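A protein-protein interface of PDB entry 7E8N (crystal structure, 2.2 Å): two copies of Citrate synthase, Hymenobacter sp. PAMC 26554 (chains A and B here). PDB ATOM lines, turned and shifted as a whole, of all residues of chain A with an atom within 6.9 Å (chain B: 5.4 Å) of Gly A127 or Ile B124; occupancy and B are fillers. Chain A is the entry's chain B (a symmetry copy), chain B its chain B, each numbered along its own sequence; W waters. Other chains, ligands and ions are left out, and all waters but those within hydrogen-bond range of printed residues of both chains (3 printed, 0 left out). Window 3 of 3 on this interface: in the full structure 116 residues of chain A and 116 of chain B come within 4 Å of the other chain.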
ATOM      1  N   ASP A 120     -26.705  11.740 -17.000  1.00  0.00           N
ATOM      2  CA  ASP A 120     -25.823  12.180 -15.876  1.00  0.00           C
ATOM      3  C   ASP A 120     -26.255  13.547 -15.335  1.00  0.00           C
ATOM      4  O   ASP A 120     -26.067  13.746 -14.108  1.00  0.00           O
ATOM      5  CB  ASP A 120     -24.358  12.142 -16.248  1.00  0.00           C
ATOM      6  CG  ASP A 120     -23.819  10.720 -16.290  1.00  0.00           C
ATOM      7  OD1 ASP A 120     -24.365   9.874 -15.562  1.00  0.00           O
ATOM      8  OD2 ASP A 120     -22.859  10.478 -17.058  1.00  0.00           O
ATOM      9  N   ARG A 122     -29.369  14.638 -15.247  1.00  0.00           N
ATOM     10  CA  ARG A 122     -30.566  14.277 -14.442  1.00  0.00           C
ATOM     11  C   ARG A 122     -30.117  13.754 -13.063  1.00  0.00           C
ATOM     12  O   ARG A 122     -30.746  14.065 -12.056  1.00  0.00           O
ATOM     13  CB  ARG A 122     -31.442  13.279 -15.207  1.00  0.00           C
ATOM     14  CG  ARG A 122     -32.722  12.903 -14.480  1.00  0.00           C
ATOM     15  CD  ARG A 122     -32.530  11.789 -13.473  1.00  0.00           C
ATOM     16  NE  ARG A 122     -32.266  10.534 -14.156  1.00  0.00           N
ATOM     17  CZ  ARG A 122     -31.897   9.401 -13.576  1.00  0.00           C
ATOM     18  NH1 ARG A 122     -31.726   9.325 -12.258  1.00  0.00           N
ATOM     19  NH2 ARG A 122     -31.699   8.344 -14.341  1.00  0.00           N
ATOM     20  N   LYS A 123     -29.057  12.985 -13.010  1.00  0.00           N
ATOM     21  CA  LYS A 123     -28.530  12.437 -11.736  1.00  0.00           C
ATOM     22  C   LYS A 123     -27.903  13.543 -10.867  1.00  0.00           C
ATOM     23  O   LYS A 123     -28.150  13.484  -9.700  1.00  0.00           O
ATOM     24  CB  LYS A 123     -27.556  11.303 -12.061  1.00  0.00           C
ATOM     25  CG  LYS A 123     -28.230  10.123 -12.752  1.00  0.00           C
ATOM     26  CD  LYS A 123     -27.306   8.958 -12.976  1.00  0.00           C
ATOM     27  CE  LYS A 123     -28.067   7.692 -13.296  1.00  0.00           C
ATOM     28  NZ  LYS A 123     -27.112   6.609 -13.589  1.00  0.00           N
ATOM     29  N   ILE A 124     -27.123  14.490 -11.417  1.00  0.00           N
ATOM     30  CA  ILE A 124     -26.725  15.748 -10.701  1.00  0.00           C
ATOM     31  C   ILE A 124     -27.993  16.436 -10.170  1.00  0.00           C
ATOM     32  O   ILE A 124     -28.076  16.644  -8.967  1.00  0.00           O
ATOM     33  CB  ILE A 124     -25.900  16.724 -11.562  1.00  0.00           C
ATOM     34  CG1 ILE A 124     -24.561  16.125 -11.983  1.00  0.00           C
ATOM     35  CG2 ILE A 124     -25.712  18.050 -10.832  1.00  0.00           C
ATOM     36  CD1 ILE A 124     -23.923  16.823 -13.177  1.00  0.00           C
ATOM     37  N   PHE A 125     -28.986  16.692 -11.016  1.00  0.00           N
ATOM     38  CA  PHE A 125     -30.307  17.260 -10.606  1.00  0.00           C
ATOM     39  C   PHE A 125     -30.914  16.478  -9.431  1.00  0.00           C
ATOM     40  O   PHE A 125     -31.474  17.117  -8.485  1.00  0.00           O
ATOM     41  CB  PHE A 125     -31.292  17.279 -11.781  1.00  0.00           C
ATOM     42  CG  PHE A 125     -32.722  17.533 -11.396  1.00  0.00           C
ATOM     43  CD1 PHE A 125     -33.165  18.812 -11.098  1.00  0.00           C
ATOM     44  CD2 PHE A 125     -33.613  16.481 -11.236  1.00  0.00           C
ATOM     45  CE1 PHE A 125     -34.480  19.045 -10.720  1.00  0.00           C
ATOM     46  CE2 PHE A 125     -34.923  16.711 -10.840  1.00  0.00           C
ATOM     47  CZ  PHE A 125     -35.364  17.995 -10.604  1.00  0.00           C
ATOM     48  N   ASP A 126     -30.819  15.144  -9.450  1.00  0.00           N
ATOM     49  CA  ASP A 126     -31.353  14.294  -8.358  1.00  0.00           C
ATOM     50  C   ASP A 126     -30.856  14.786  -6.980  1.00  0.00           C
ATOM     51  O   ASP A 126     -31.564  14.530  -6.001  1.00  0.00           O
ATOM     52  CB  ASP A 126     -31.007  12.820  -8.561  1.00  0.00           C
ATOM     53  CG  ASP A 126     -31.996  12.054  -9.427  1.00  0.00           C
ATOM     54  OD1 ASP A 126     -33.205  12.208  -9.197  1.00  0.00           O
ATOM     55  OD2 ASP A 126     -31.547  11.295 -10.312  1.00  0.00           O
ATOM     56  N   GLY A 127     -29.678  15.415  -6.885  1.00  0.00           N
ATOM     57  CA  GLY A 127     -29.070  15.749  -5.584  1.00  0.00           C
ATOM     58  C   GLY A 127     -29.755  16.919  -4.900  1.00  0.00           C
ATOM     59  O   GLY A 127     -29.580  17.081  -3.706  1.00  0.00           O
ATOM     60  N   PHE A 128     -30.490  17.725  -5.643  1.00  0.00           N
ATOM     61  CA  PHE A 128     -31.070  18.989  -5.134  1.00  0.00           C
ATOM     62  C   PHE A 128     -32.338  18.676  -4.368  1.00  0.00           C
ATOM     63  O   PHE A 128     -33.265  18.077  -4.892  1.00  0.00           O
ATOM     64  CB  PHE A 128     -31.400  19.975  -6.243  1.00  0.00           C
ATOM     65  CG  PHE A 128     -30.225  20.711  -6.814  1.00  0.00           C
ATOM     66  CD1 PHE A 128     -29.737  21.853  -6.205  1.00  0.00           C
ATOM     67  CD2 PHE A 128     -29.630  20.276  -7.977  1.00  0.00           C
ATOM     68  CE1 PHE A 128     -28.675  22.538  -6.760  1.00  0.00           C
ATOM     69  CE2 PHE A 128     -28.532  20.938  -8.499  1.00  0.00           C
ATOM     70  CZ  PHE A 128     -28.073  22.081  -7.903  1.00  0.00           C
ATOM     71  N   PRO A 129     -32.400  19.079  -3.093  1.00  0.00           N
ATOM     72  CA  PRO A 129     -33.638  18.991  -2.329  1.00  0.00           C
ATOM     73  C   PRO A 129     -34.788  19.719  -3.021  1.00  0.00           C
ATOM     74  O   PRO A 129     -34.558  20.737  -3.642  1.00  0.00           O
ATOM     75  CB  PRO A 129     -33.339  19.737  -1.014  1.00  0.00           C
ATOM     76  CG  PRO A 129     -31.824  19.707  -0.908  1.00  0.00           C
ATOM     77  CD  PRO A 129     -31.300  19.671  -2.334  1.00  0.00           C
ATOM     78  N   SER A 130     -36.002  19.218  -2.834  1.00  0.00           N
ATOM     79  CA  SER A 130     -37.257  19.810  -3.352  1.00  0.00           C
ATOM     80  C   SER A 130     -37.403  21.275  -2.898  1.00  0.00           C
ATOM     81  O   SER A 130     -38.007  22.037  -3.634  1.00  0.00           O
ATOM     82  CB  SER A 130     -38.436  18.991  -2.896  1.00  0.00           C
ATOM     83  OG  SER A 130     -38.592  19.120  -1.480  1.00  0.00           O
ATOM     84  N   THR A 132     -35.072  23.565  -2.699  1.00  0.00           N
ATOM     85  CA  THR A 132     -34.106  24.452  -3.380  1.00  0.00           C
ATOM     86  C   THR A 132     -34.840  25.435  -4.294  1.00  0.00           C
ATOM     87  O   THR A 132     -35.655  25.004  -5.102  1.00  0.00           O
ATOM     88  CB  THR A 132     -33.148  23.660  -4.266  1.00  0.00           C
ATOM     89  OG1 THR A 132     -32.555  22.681  -3.436  1.00  0.00           O
ATOM     90  CG2 THR A 132     -32.091  24.526  -4.900  1.00  0.00           C
ATOM     91  N   SER A 140     -26.963  26.348 -11.711  1.00  0.00           N
ATOM     92  CA  SER A 140     -26.040  25.229 -11.421  1.00  0.00           C
ATOM     93  C   SER A 140     -25.999  24.208 -12.567  1.00  0.00           C
ATOM     94  O   SER A 140     -24.926  23.838 -12.972  1.00  0.00           O
ATOM     95  CB  SER A 140     -26.381  24.625 -10.110  1.00  0.00           C
ATOM     96  OG  SER A 140     -25.710  23.413  -9.951  1.00  0.00           O
ATOM     97  N   LEU A 141     -27.143  23.801 -13.085  1.00  0.00           N
ATOM     98  CA  LEU A 141     -27.157  22.823 -14.190  1.00  0.00           C
ATOM     99  C   LEU A 141     -26.623  23.493 -15.462  1.00  0.00           C
ATOM    100  O   LEU A 141     -25.933  22.838 -16.216  1.00  0.00           O
ATOM    101  CB  LEU A 141     -28.573  22.267 -14.347  1.00  0.00           C
ATOM    102  CG  LEU A 141     -29.044  21.356 -13.212  1.00  0.00           C
ATOM    103  CD1 LEU A 141     -30.372  20.719 -13.545  1.00  0.00           C
ATOM    104  CD2 LEU A 141     -28.012  20.290 -12.899  1.00  0.00           C
ATOM    105  N   ASN A 183     -39.268  19.640  -9.396  1.00  0.00           N
ATOM    106  CA  ASN A 183     -38.457  19.440  -8.178  1.00  0.00           C
ATOM    107  C   ASN A 183     -39.212  20.030  -6.978  1.00  0.00           C
ATOM    108  O   ASN A 183     -39.367  19.308  -6.000  1.00  0.00           O
ATOM    109  CB  ASN A 183     -37.055  20.020  -8.309  1.00  0.00           C
ATOM    110  CG  ASN A 183     -36.168  19.586  -7.161  1.00  0.00           C
ATOM    111  OD1 ASN A 183     -35.932  18.397  -6.967  1.00  0.00           O
ATOM    112  ND2 ASN A 183     -35.710  20.535  -6.370  1.00  0.00           N
ATOM    113  N   GLU B 119     -24.218  17.212   3.143  1.00  0.00           N
ATOM    114  CA  GLU B 119     -24.374  15.874   2.517  1.00  0.00           C
ATOM    115  C   GLU B 119     -25.163  15.988   1.202  1.00  0.00           C
ATOM    116  O   GLU B 119     -24.771  15.297   0.216  1.00  0.00           O
ATOM    117  CB  GLU B 119     -24.947  14.889   3.545  1.00  0.00           C
ATOM    118  CG  GLU B 119     -23.852  14.347   4.461  1.00  0.00           C
ATOM    119  CD  GLU B 119     -23.097  13.223   3.783  1.00  0.00           C
ATOM    120  OE1 GLU B 119     -22.059  13.499   3.177  1.00  0.00           O
ATOM    121  OE2 GLU B 119     -23.588  12.049   3.839  1.00  0.00           O
ATOM    122  N   ASP B 120     -26.150  16.877   1.106  1.00  0.00           N
ATOM    123  CA  ASP B 120     -26.888  17.016  -0.186  1.00  0.00           C
ATOM    124  C   ASP B 120     -25.978  17.571  -1.286  1.00  0.00           C
ATOM    125  O   ASP B 120     -26.214  17.177  -2.457  1.00  0.00           O
ATOM    126  CB  ASP B 120     -28.165  17.812  -0.035  1.00  0.00           C
ATOM    127  CG  ASP B 120     -29.257  17.010   0.655  1.00  0.00           C
ATOM    128  OD1 ASP B 120     -29.229  15.773   0.534  1.00  0.00           O
ATOM    129  OD2 ASP B 120     -30.121  17.636   1.311  1.00  0.00           O
ATOM    130  N   ILE B 121     -24.998  18.439  -0.964  1.00  0.00           N
ATOM    131  CA  ILE B 121     -24.070  18.981  -2.001  1.00  0.00           C
ATOM    132  C   ILE B 121     -23.140  17.861  -2.446  1.00  0.00           C
ATOM    133  O   ILE B 121     -22.904  17.738  -3.671  1.00  0.00           O
ATOM    134  CB  ILE B 121     -23.333  20.248  -1.560  1.00  0.00           C
ATOM    135  CG1 ILE B 121     -24.354  21.366  -1.374  1.00  0.00           C
ATOM    136  CG2 ILE B 121     -22.232  20.616  -2.557  1.00  0.00           C
ATOM    137  CD1 ILE B 121     -23.872  22.544  -0.580  1.00  0.00           C
ATOM    138  N   ARG B 122     -22.738  16.986  -1.522  1.00  0.00           N
ATOM    139  CA  ARG B 122     -21.928  15.789  -1.874  1.00  0.00           C
ATOM    140  C   ARG B 122     -22.730  14.895  -2.840  1.00  0.00           C
ATOM    141  O   ARG B 122     -22.161  14.341  -3.776  1.00  0.00           O
ATOM    142  CB  ARG B 122     -21.484  15.056  -0.604  1.00  0.00           C
ATOM    143  CG  ARG B 122     -20.597  13.851  -0.871  1.00  0.00           C
ATOM    144  CD  ARG B 122     -21.378  12.594  -1.187  1.00  0.00           C
ATOM    145  NE  ARG B 122     -22.072  12.122   0.000  1.00  0.00           N
ATOM    146  CZ  ARG B 122     -22.966  11.144   0.034  1.00  0.00           C
ATOM    147  NH1 ARG B 122     -23.318  10.492  -1.071  1.00  0.00           N
ATOM    148  NH2 ARG B 122     -23.505  10.832   1.198  1.00  0.00           N
ATOM    149  N   LYS B 123     -24.015  14.756  -2.628  1.00  0.00           N
ATOM    150  CA  LYS B 123     -24.885  13.929  -3.502  1.00  0.00           C
ATOM    151  C   LYS B 123     -25.074  14.583  -4.883  1.00  0.00           C
ATOM    152  O   LYS B 123     -25.027  13.838  -5.816  1.00  0.00           O
ATOM    153  CB  LYS B 123     -26.205  13.673  -2.772  1.00  0.00           C
ATOM    154  CG  LYS B 123     -26.029  12.854  -1.498  1.00  0.00           C
ATOM    155  CD  LYS B 123     -27.330  12.502  -0.832  1.00  0.00           C
ATOM    156  CE  LYS B 123     -27.160  11.393   0.181  1.00  0.00           C
ATOM    157  NZ  LYS B 123     -28.444  11.149   0.859  1.00  0.00           N
ATOM    158  N   ILE B 124     -25.289  15.905  -4.995  1.00  0.00           N
ATOM    159  CA  ILE B 124     -25.190  16.650  -6.293  1.00  0.00           C
ATOM    160  C   ILE B 124     -23.826  16.342  -6.936  1.00  0.00           C
ATOM    161  O   ILE B 124     -23.815  15.850  -8.056  1.00  0.00           O
ATOM    162  CB  ILE B 124     -25.392  18.171  -6.161  1.00  0.00           C
ATOM    163  CG1 ILE B 124     -26.794  18.521  -5.667  1.00  0.00           C
ATOM    164  CG2 ILE B 124     -25.077  18.869  -7.479  1.00  0.00           C
ATOM    165  CD1 ILE B 124     -26.909  19.924  -5.085  1.00  0.00           C
ATOM    166  N   PHE B 125     -22.723  16.531  -6.219  1.00  0.00           N
ATOM    167  CA  PHE B 125     -21.350  16.172  -6.690  1.00  0.00           C
ATOM    168  C   PHE B 125     -21.296  14.730  -7.217  1.00  0.00           C
ATOM    169  O   PHE B 125     -20.639  14.482  -8.277  1.00  0.00           O
ATOM    170  CB  PHE B 125     -20.314  16.356  -5.574  1.00  0.00           C
ATOM    171  CG  PHE B 125     -18.977  15.728  -5.851  1.00  0.00           C
ATOM    172  CD1 PHE B 125     -18.065  16.337  -6.698  1.00  0.00           C
ATOM    173  CD2 PHE B 125     -18.659  14.478  -5.339  1.00  0.00           C
ATOM    174  CE1 PHE B 125     -16.838  15.748  -6.972  1.00  0.00           C
ATOM    175  CE2 PHE B 125     -17.441  13.880  -5.627  1.00  0.00           C
ATOM    176  CZ  PHE B 125     -16.520  14.523  -6.427  1.00  0.00           C
ATOM    177  N   ASP B 126     -21.958  13.789  -6.535  1.00  0.00           N
ATOM    178  CA  ASP B 126     -21.988  12.369  -6.967  1.00  0.00           C
ATOM    179  C   ASP B 126     -22.392  12.251  -8.453  1.00  0.00           C
ATOM    180  O   ASP B 126     -21.996  11.256  -9.067  1.00  0.00           O
ATOM    181  CB  ASP B 126     -22.911  11.526  -6.088  1.00  0.00           C
ATOM    182  CG  ASP B 126     -22.251  10.967  -4.836  1.00  0.00           C
ATOM    183  OD1 ASP B 126     -21.136  10.440  -4.956  1.00  0.00           O
ATOM    184  OD2 ASP B 126     -22.870  11.047  -3.753  1.00  0.00           O
ATOM    185  N   GLY B 127     -23.182  13.182  -9.003  1.00  0.00           N
ATOM    186  CA  GLY B 127     -23.744  13.034 -10.357  1.00  0.00           C
ATOM    187  C   GLY B 127     -22.712  13.259 -11.449  1.00  0.00           C
ATOM    188  O   GLY B 127     -22.948  12.849 -12.570  1.00  0.00           O
ATOM    189  N   PHE B 128     -21.612  13.917 -11.131  1.00  0.00           N
ATOM    190  CA  PHE B 128     -20.611  14.347 -12.134  1.00  0.00           C
ATOM    191  C   PHE B 128     -19.712  13.175 -12.468  1.00  0.00           C
ATOM    192  O   PHE B 128     -19.080  12.593 -11.600  1.00  0.00           O
ATOM    193  CB  PHE B 128     -19.749  15.501 -11.649  1.00  0.00           C
ATOM    194  CG  PHE B 128     -20.405  16.848 -11.685  1.00  0.00           C
ATOM    195  CD1 PHE B 128     -20.422  17.600 -12.845  1.00  0.00           C
ATOM    196  CD2 PHE B 128     -20.978  17.375 -10.548  1.00  0.00           C
ATOM    197  CE1 PHE B 128     -21.001  18.853 -12.855  1.00  0.00           C
ATOM    198  CE2 PHE B 128     -21.604  18.608 -10.579  1.00  0.00           C
ATOM    199  CZ  PHE B 128     -21.593  19.355 -11.725  1.00  0.00           C
ATOM    200  N   LEU B 141     -21.021  23.671  -8.302  1.00  0.00           N
ATOM    201  CA  LEU B 141     -21.292  23.499  -6.861  1.00  0.00           C
ATOM    202  C   LEU B 141     -21.317  24.875  -6.186  1.00  0.00           C
ATOM    203  O   LEU B 141     -22.122  25.070  -5.297  1.00  0.00           O
ATOM    204  CB  LEU B 141     -20.251  22.550  -6.266  1.00  0.00           C
ATOM    205  CG  LEU B 141     -20.370  21.092  -6.710  1.00  0.00           C
ATOM    206  CD1 LEU B 141     -19.419  20.211  -5.936  1.00  0.00           C
ATOM    207  CD2 LEU B 141     -21.792  20.588  -6.567  1.00  0.00           C
ATOM    208  N   ALA B 144     -24.728  26.352  -6.483  1.00  0.00           N
ATOM    209  CA  ALA B 144     -25.720  25.606  -5.687  1.00  0.00           C
ATOM    210  C   ALA B 144     -25.798  26.144  -4.246  1.00  0.00           C
ATOM    211  O   ALA B 144     -26.846  26.034  -3.668  1.00  0.00           O
ATOM    212  CB  ALA B 144     -25.390  24.144  -5.716  1.00  0.00           C
ATOM    213  N   PHE B 148     -28.783  26.376  -0.954  1.00  0.00           N
ATOM    214  CA  PHE B 148     -28.705  25.814   0.415  1.00  0.00           C
ATOM    215  C   PHE B 148     -28.724  26.917   1.481  1.00  0.00           C
ATOM    216  O   PHE B 148     -29.137  26.642   2.569  1.00  0.00           O
ATOM    217  CB  PHE B 148     -27.520  24.857   0.529  1.00  0.00           C
ATOM    218  CG  PHE B 148     -27.713  23.569  -0.224  1.00  0.00           C
ATOM    219  CD1 PHE B 148     -27.489  23.501  -1.581  1.00  0.00           C
ATOM    220  CD2 PHE B 148     -28.165  22.433   0.413  1.00  0.00           C
ATOM    221  CE1 PHE B 148     -27.703  22.333  -2.282  1.00  0.00           C
ATOM    222  CE2 PHE B 148     -28.380  21.265  -0.292  1.00  0.00           C
ATOM    223  CZ  PHE B 148     -28.135  21.212  -1.635  1.00  0.00           C
HETATM  224  O   HOH W   1     -26.808  12.775  -7.500  1.00  0.00           O
HETATM  225  O   HOH W   2     -24.044  10.585 -12.884  1.00  0.00           O
HETATM  226  O   HOH W   3     -29.545  15.081  -2.149  1.00  0.00           O
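Of the printed residues of chain B, Gly A127 touches Asp B120 (3.6 Å) and Ile B124 (3.5 Å).
Printed residues of chain A within 4 Å of Ala B144: Phe A128.
Printed residues of chain A within 4 Å of Phe B148: Pro A129 (3.6 Å).
Of the printed residues of chain B, Phe A128 touches Ile B124 and Ala B144.
Printed residues of chain B within 4 Å of Asp A120: Gly B127.
Ile B121 touches none of the printed residues of chain A.
Arg B122 touches none of the printed residues of chain A.
The nearest residue of chain B that does not touch Gly A127 is Lys B123 (4.2 Å).
The nearest printed residue of chain A that does not touch Ile B124 is Pro A129 (5.2 Å).
The nearest printed residue of chain A that does not touch Gly B127 is Lys A123 (4.2 Å).
Asp A120 touches Gly B127, and with the chains exchanged Gly A127 touches Asp B120.
Ile B124 touches its own counterpart, Ile A124.
Ile A124 touches Gly B127, and with the chains exchanged Gly A127 touches Ile B124.
Ile A124 touches Phe B128, and with the chains exchanged Phe A128 touches Ile B124.
Positions printed for both chains: 120, 122, 123, 124, 125, 126, 127, 128 and 141.
Of the 10 pairs that touch across the chains among the printed residues, 7 have their exchanged pair printed and touching as well.
The backbone carbonyl oxygen (O) of Phe A128 sits close to the side-chain amide oxygen (OD1) of Asn A183, 3.4 Å away.
The side-chain hydroxyl (OG1) of Thr A132 lies within hydrogen-bond range of the backbone carbonyl oxygen (O) of Pro A129 (2.8 Å).
O of Pro A129 sits at hydrogen-bond distance from ND2 of Asn A183, 3.0 Å away.
Water W2 lies within hydrogen-bond range of the backbone carbonyl oxygen of Gly B127 (2.5 Å) and the side-chain carboxylate of Asp A120 (2.8 Å).
Water W3 bridges the backbone carbonyl oxygen of Gly A127 (2.5 Å) and the side-chain carboxylate of Asp B120 (2.8 Å).
Water W1 bridges O of Lys B123 (2.7 Å) and O of Lys A123 (2.7 Å).
Among the printed residues, merely in contact across the chains: Asp A120 with Gly B127, Ile A124 with Ile B124, Ile A124 with Gly B127, Ile A124 with Phe B128, Gly A127 with Asp B120, Gly A127 with Ile B124, Phe A128 with Ile B124, Phe A128 with Ala B144, Pro A129 with Asp B120 and Pro A129 with Phe B148.
Printed residues of chain A that touch a printed residue of chain B: Asp A120, Ile A124, Gly A127, Phe A128 and Pro A129.
Of the 13 printed residues of chain B, 6 touch a printed residue of chain A.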
